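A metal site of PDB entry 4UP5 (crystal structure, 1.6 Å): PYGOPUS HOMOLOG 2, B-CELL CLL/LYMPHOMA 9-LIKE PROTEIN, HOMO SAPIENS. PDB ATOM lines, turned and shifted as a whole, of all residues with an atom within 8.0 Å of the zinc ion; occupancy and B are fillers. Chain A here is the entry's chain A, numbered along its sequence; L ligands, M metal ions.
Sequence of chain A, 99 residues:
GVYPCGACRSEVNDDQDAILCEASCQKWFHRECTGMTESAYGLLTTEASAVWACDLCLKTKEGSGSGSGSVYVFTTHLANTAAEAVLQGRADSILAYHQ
Within 4 Å of the zinc ion: Cys 5, Cys 8, His 30 and Cys 33.
O of Glu 11 sits at hydrogen-bond distance from NE2 of His 30, 3.0 Å away.
A ring nitrogen (NE2) of His 30 lies within hydrogen-bond range of the side-chain amide oxygen of Gln 16, 3.0 Å away.
The side-chain sulfur (SG) of Cys 8 sits close to the backbone NH (N) of Ser 10 (3.5 Å).
The side-chain sulfur (SG) of Cys 5 lies close to the backbone NH (N) of Ala 7 (3.4 Å).
The backbone carbonyl oxygen (O) of Ser 10 sits at hydrogen-bond distance from the backbone NH (N) of Cys 5, at 2.8 Å.
The zinc ion is bound by a ring nitrogen (ND1) of His 30, the side-chain sulfur (SG) of Cys 33, the side-chain sulfur (SG) of Cys 8 and the side-chain sulfur (SG) of Cys 5.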
ATOM      1  N   PRO A   4      12.073  -7.179  -1.190  1.00  0.00           N
ATOM      2  CA  PRO A   4      12.929  -7.005  -0.037  1.00  0.00           C
ATOM      3  C   PRO A   4      14.402  -6.814  -0.421  1.00  0.00           C
ATOM      4  O   PRO A   4      14.878  -7.344  -1.457  1.00  0.00           O
ATOM      5  CB  PRO A   4      12.844  -8.344   0.683  1.00  0.00           C
ATOM      6  CG  PRO A   4      12.545  -9.283  -0.471  1.00  0.00           C
ATOM      7  CD  PRO A   4      11.810  -8.585  -1.488  1.00  0.00           C
ATOM      8  N   CYS A   5      15.111  -6.033   0.389  1.00  0.00           N
ATOM      9  CA  CYS A   5      16.505  -5.754   0.117  1.00  0.00           C
ATOM     10  C   CYS A   5      17.333  -7.023   0.219  1.00  0.00           C
ATOM     11  O   CYS A   5      17.252  -7.771   1.242  1.00  0.00           O
ATOM     12  CB  CYS A   5      17.025  -4.676   1.110  1.00  0.00           C
ATOM     13  SG  CYS A   5      18.792  -4.345   0.982  1.00  0.00           S
ATOM     14  N   GLY A   6      18.173  -7.281  -0.799  1.00  0.00           N
ATOM     15  CA  GLY A   6      19.120  -8.359  -0.816  1.00  0.00           C
ATOM     16  C   GLY A   6      20.071  -8.477   0.337  1.00  0.00           C
ATOM     17  O   GLY A   6      20.610  -9.553   0.637  1.00  0.00           O
ATOM     18  N   ALA A   7      20.357  -7.333   0.949  1.00  0.00           N
ATOM     19  CA  ALA A   7      21.242  -7.301   2.076  1.00  0.00           C
ATOM     20  C   ALA A   7      20.573  -7.319   3.394  1.00  0.00           C
ATOM     21  O   ALA A   7      20.825  -8.206   4.221  1.00  0.00           O
ATOM     22  CB  ALA A   7      22.129  -6.070   1.953  1.00  0.00           C
ATOM     23  N   CYS A   8      19.633  -6.421   3.657  1.00  0.00           N
ATOM     24  CA  CYS A   8      19.142  -6.324   4.995  1.00  0.00           C
ATOM     25  C   CYS A   8      17.806  -7.088   5.201  1.00  0.00           C
ATOM     26  O   CYS A   8      17.263  -7.196   6.316  1.00  0.00           O
ATOM     27  CB  CYS A   8      18.896  -4.856   5.318  1.00  0.00           C
ATOM     28  SG  CYS A   8      17.557  -3.988   4.544  1.00  0.00           S
ATOM     29  N   ARG A   9      17.253  -7.468   4.074  1.00  0.00           N
ATOM     30  CA  ARG A   9      15.942  -8.182   4.026  1.00  0.00           C
ATOM     31  C   ARG A   9      14.677  -7.429   4.341  1.00  0.00           C
ATOM     32  O   ARG A   9      13.623  -8.084   4.421  1.00  0.00           O
ATOM     33  CB  ARG A   9      16.015  -9.415   4.859  1.00  0.00           C
ATOM     34  CG  ARG A   9      17.142 -10.354   4.433  1.00  0.00           C
ATOM     35  CD  ARG A   9      17.064 -10.781   2.998  1.00  0.00           C
ATOM     36  NE  ARG A   9      17.794 -12.051   2.892  1.00  0.00           N
ATOM     37  CZ  ARG A   9      18.168 -12.653   1.773  1.00  0.00           C
ATOM     38  NH1 ARG A   9      17.886 -12.117   0.581  1.00  0.00           N
ATOM     39  NH2 ARG A   9      18.845 -13.815   1.876  1.00  0.00           N
ATOM     40  N   SER A  10      14.776  -6.117   4.531  1.00  0.00           N
ATOM     41  CA  SER A  10      13.661  -5.255   4.743  1.00  0.00           C
ATOM     42  C   SER A  10      13.165  -4.670   3.462  1.00  0.00           C
ATOM     43  O   SER A  10      13.928  -4.569   2.445  1.00  0.00           O
ATOM     44  CB  SER A  10      14.186  -4.189   5.732  1.00  0.00           C
ATOM     45  OG  SER A  10      13.198  -3.443   6.295  1.00  0.00           O
ATOM     46  N   GLU A  11      11.921  -4.198   3.423  1.00  0.00           N
ATOM     47  CA  GLU A  11      11.318  -3.733   2.171  1.00  0.00           C
ATOM     48  C   GLU A  11      12.086  -2.564   1.579  1.00  0.00           C
ATOM     49  O   GLU A  11      12.560  -1.678   2.323  1.00  0.00           O
ATOM     50  CB  GLU A  11       9.837  -3.287   2.297  1.00  0.00           C
ATOM     51  CG  GLU A  11       9.560  -2.152   3.181  1.00  0.00           C
ATOM     52  CD  GLU A  11       8.093  -1.644   3.125  1.00  0.00           C
ATOM     53  OE1 GLU A  11       7.287  -2.189   2.332  1.00  0.00           O
ATOM     54  OE2 GLU A  11       7.793  -0.705   3.922  1.00  0.00           O
ATOM     55  N   VAL A  12      12.106  -2.540   0.246  1.00  0.00           N
ATOM     56  CA  VAL A  12      12.640  -1.440  -0.575  1.00  0.00           C
ATOM     57  C   VAL A  12      11.414  -0.615  -0.988  1.00  0.00           C
ATOM     58  O   VAL A  12      10.563  -1.056  -1.742  1.00  0.00           O
ATOM     59  CB  VAL A  12      13.461  -1.946  -1.783  1.00  0.00           C
ATOM     60  CG1 VAL A  12      13.832  -0.756  -2.693  1.00  0.00           C
ATOM     61  CG2 VAL A  12      14.673  -2.698  -1.339  1.00  0.00           C
ATOM     62  N   GLN A  16      13.207   5.316  -1.398  1.00  0.00           N
ATOM     63  CA  GLN A  16      14.623   5.010  -1.044  1.00  0.00           C
ATOM     64  C   GLN A  16      15.448   4.757  -2.336  1.00  0.00           C
ATOM     65  O   GLN A  16      14.918   4.193  -3.328  1.00  0.00           O
ATOM     66  CB  GLN A  16      14.644   3.734  -0.187  1.00  0.00           C
ATOM     67  CG  GLN A  16      13.858   3.902   1.121  1.00  0.00           C
ATOM     68  CD  GLN A  16      13.765   2.595   1.831  1.00  0.00           C
ATOM     69  OE1 GLN A  16      13.402   1.601   1.202  1.00  0.00           O
ATOM     70  NE2 GLN A  16      14.056   2.582   3.125  1.00  0.00           N
ATOM     71  N   ASP A  17      16.738   5.160  -2.327  1.00  0.00           N
ATOM     72  CA  ASP A  17      17.647   4.879  -3.395  1.00  0.00           C
ATOM     73  C   ASP A  17      17.831   3.336  -3.394  1.00  0.00           C
ATOM     74  O   ASP A  17      18.180   2.781  -2.364  1.00  0.00           O
ATOM     75  CB  ASP A  17      19.047   5.451  -3.096  1.00  0.00           C
ATOM     76  CG  ASP A  17      19.127   6.968  -3.166  1.00  0.00           C
ATOM     77  OD1 ASP A  17      18.133   7.593  -3.602  1.00  0.00           O
ATOM     78  OD2 ASP A  17      20.206   7.545  -2.743  1.00  0.00           O
ATOM     79  N   TRP A  28      16.817  -6.590  -5.508  1.00  0.00           N
ATOM     80  CA  TRP A  28      16.900  -5.111  -5.322  1.00  0.00           C
ATOM     81  C   TRP A  28      17.616  -4.965  -4.003  1.00  0.00           C
ATOM     82  O   TRP A  28      17.401  -5.731  -3.047  1.00  0.00           O
ATOM     83  CB  TRP A  28      15.532  -4.454  -5.238  1.00  0.00           C
ATOM     84  CG  TRP A  28      14.934  -4.218  -6.562  1.00  0.00           C
ATOM     85  CD1 TRP A  28      14.082  -5.092  -7.260  1.00  0.00           C
ATOM     86  CD2 TRP A  28      15.210  -3.144  -7.438  1.00  0.00           C
ATOM     87  NE1 TRP A  28      13.766  -4.536  -8.464  1.00  0.00           N
ATOM     88  CE2 TRP A  28      14.445  -3.361  -8.621  1.00  0.00           C
ATOM     89  CE3 TRP A  28      15.962  -1.969  -7.327  1.00  0.00           C
ATOM     90  CZ2 TRP A  28      14.461  -2.489  -9.670  1.00  0.00           C
ATOM     91  CZ3 TRP A  28      15.989  -1.071  -8.406  1.00  0.00           C
ATOM     92  CH2 TRP A  28      15.204  -1.334  -9.559  1.00  0.00           C
ATOM     93  N   PHE A  29      18.430  -3.878  -3.929  1.00  0.00           N
ATOM     94  CA  PHE A  29      19.115  -3.585  -2.697  1.00  0.00           C
ATOM     95  C   PHE A  29      18.960  -2.082  -2.369  1.00  0.00           C
ATOM     96  O   PHE A  29      19.011  -1.209  -3.272  1.00  0.00           O
ATOM     97  CB  PHE A  29      20.630  -3.830  -2.856  1.00  0.00           C
ATOM     98  CG  PHE A  29      21.042  -5.275  -2.887  1.00  0.00           C
ATOM     99  CD1 PHE A  29      20.747  -6.042  -3.982  1.00  0.00           C
ATOM    100  CD2 PHE A  29      21.804  -5.805  -1.864  1.00  0.00           C
ATOM    101  CE1 PHE A  29      21.143  -7.373  -4.032  1.00  0.00           C
ATOM    102  CE2 PHE A  29      22.190  -7.132  -1.891  1.00  0.00           C
ATOM    103  CZ  PHE A  29      21.863  -7.879  -3.042  1.00  0.00           C
ATOM    104  N   HIS A  30      18.864  -1.728  -1.092  1.00  0.00           N
ATOM    105  CA  HIS A  30      19.013  -0.305  -0.768  1.00  0.00           C
ATOM    106  C   HIS A  30      20.360   0.137  -1.100  1.00  0.00           C
ATOM    107  O   HIS A  30      21.303  -0.510  -0.699  1.00  0.00           O
ATOM    108  CB  HIS A  30      18.828  -0.101   0.767  1.00  0.00           C
ATOM    109  CG  HIS A  30      17.473  -0.461   1.260  1.00  0.00           C
ATOM    110  ND1 HIS A  30      17.254  -1.534   2.117  1.00  0.00           N
ATOM    111  CD2 HIS A  30      16.274   0.151   1.094  1.00  0.00           C
ATOM    112  CE1 HIS A  30      15.951  -1.538   2.440  1.00  0.00           C
ATOM    113  NE2 HIS A  30      15.343  -0.565   1.812  1.00  0.00           N
ATOM    114  N   ARG A  31      20.523   1.310  -1.732  1.00  0.00           N
ATOM    115  CA  ARG A  31      21.829   1.844  -1.985  1.00  0.00           C
ATOM    116  C   ARG A  31      22.673   1.883  -0.673  1.00  0.00           C
ATOM    117  O   ARG A  31      23.821   1.417  -0.621  1.00  0.00           O
ATOM    118  CB  ARG A  31      21.729   3.252  -2.572  1.00  0.00           C
ATOM    119  CG  ARG A  31      23.117   3.882  -2.794  1.00  0.00           C
ATOM    120  CD  ARG A  31      23.039   5.392  -2.999  1.00  0.00           C
ATOM    121  NE  ARG A  31      22.555   6.171  -1.881  1.00  0.00           N
ATOM    122  CZ  ARG A  31      23.276   6.424  -0.817  1.00  0.00           C
ATOM    123  NH1 ARG A  31      24.541   6.038  -0.687  1.00  0.00           N
ATOM    124  NH2 ARG A  31      22.721   7.145   0.175  1.00  0.00           N
ATOM    125  N   GLU A  32      22.086   2.366   0.438  1.00  0.00           N
ATOM    126  CA  GLU A  32      22.871   2.461   1.693  1.00  0.00           C
ATOM    127  C   GLU A  32      23.274   1.128   2.280  1.00  0.00           C
ATOM    128  O   GLU A  32      24.303   1.026   2.927  1.00  0.00           O
ATOM    129  CB  GLU A  32      22.078   3.221   2.756  1.00  0.00           C
ATOM    130  CG  GLU A  32      21.857   4.704   2.377  1.00  0.00           C
ATOM    131  CD  GLU A  32      20.921   5.474   3.352  1.00  0.00           C
ATOM    132  OE1 GLU A  32      20.565   4.904   4.422  1.00  0.00           O
ATOM    133  OE2 GLU A  32      20.534   6.626   3.047  1.00  0.00           O
ATOM    134  N   CYS A  33      22.569   0.036   1.971  1.00  0.00           N
ATOM    135  CA  CYS A  33      23.080  -1.240   2.408  1.00  0.00           C
ATOM    136  C   CYS A  33      24.295  -1.834   1.679  1.00  0.00           C
ATOM    137  O   CYS A  33      24.904  -2.867   2.028  1.00  0.00           O
ATOM    138  CB  CYS A  33      21.873  -2.205   2.325  1.00  0.00           C
ATOM    139  SG  CYS A  33      20.576  -1.839   3.572  1.00  0.00           S
ATOM    140  N   THR A  34      24.600  -1.265   0.538  1.00  0.00           N
ATOM    141  CA  THR A  34      25.630  -1.796  -0.300  1.00  0.00           C
ATOM    142  C   THR A  34      26.958  -1.120  -0.072  1.00  0.00           C
ATOM    143  O   THR A  34      27.984  -1.648  -0.444  1.00  0.00           O
ATOM    144  CB  THR A  34      25.341  -1.623  -1.790  1.00  0.00           C
ATOM    145  OG1 THR A  34      25.301  -0.222  -2.127  1.00  0.00           O
ATOM    146  CG2 THR A  34      23.925  -2.342  -2.117  1.00  0.00           C
HETATM  147  C1  LIG L   1      24.861  -8.909   1.223  1.00  0.00           C
HETATM  148  O1  LIG L   1      24.431  -9.624   2.320  1.00  0.00           O
HETATM  149  C2  LIG L   1      23.773  -8.909   3.350  1.00  0.00           C
HETATM  150  C3  LIG L   1      25.466  -7.684   1.411  1.00  0.00           C
HETATM  151  C4  LIG L   1      25.879  -6.987   0.291  1.00  0.00           C
HETATM  152  C5  LIG L   1      25.696  -7.489  -1.003  1.00  0.00           C
HETATM  153  C6  LIG L   1      25.082  -8.731  -1.156  1.00  0.00           C
HETATM  154  C7  LIG L   1      24.666  -9.437  -0.040  1.00  0.00           C
HETATM  155  N1  LIG L   1      26.171  -6.684  -2.034  1.00  0.00           N
HETATM  156  C8  LIG L   1      26.696  -5.584  -1.551  1.00  0.00           C
HETATM  157  N2  LIG L   1      27.226  -4.612  -2.296  1.00  0.00           N
HETATM  158  S1  LIG L   1      26.671  -5.434   0.204  1.00  0.00           S
HETATM  159 ZN    ZN M   1      18.666  -2.854   2.844  1.00  0.00          ZN
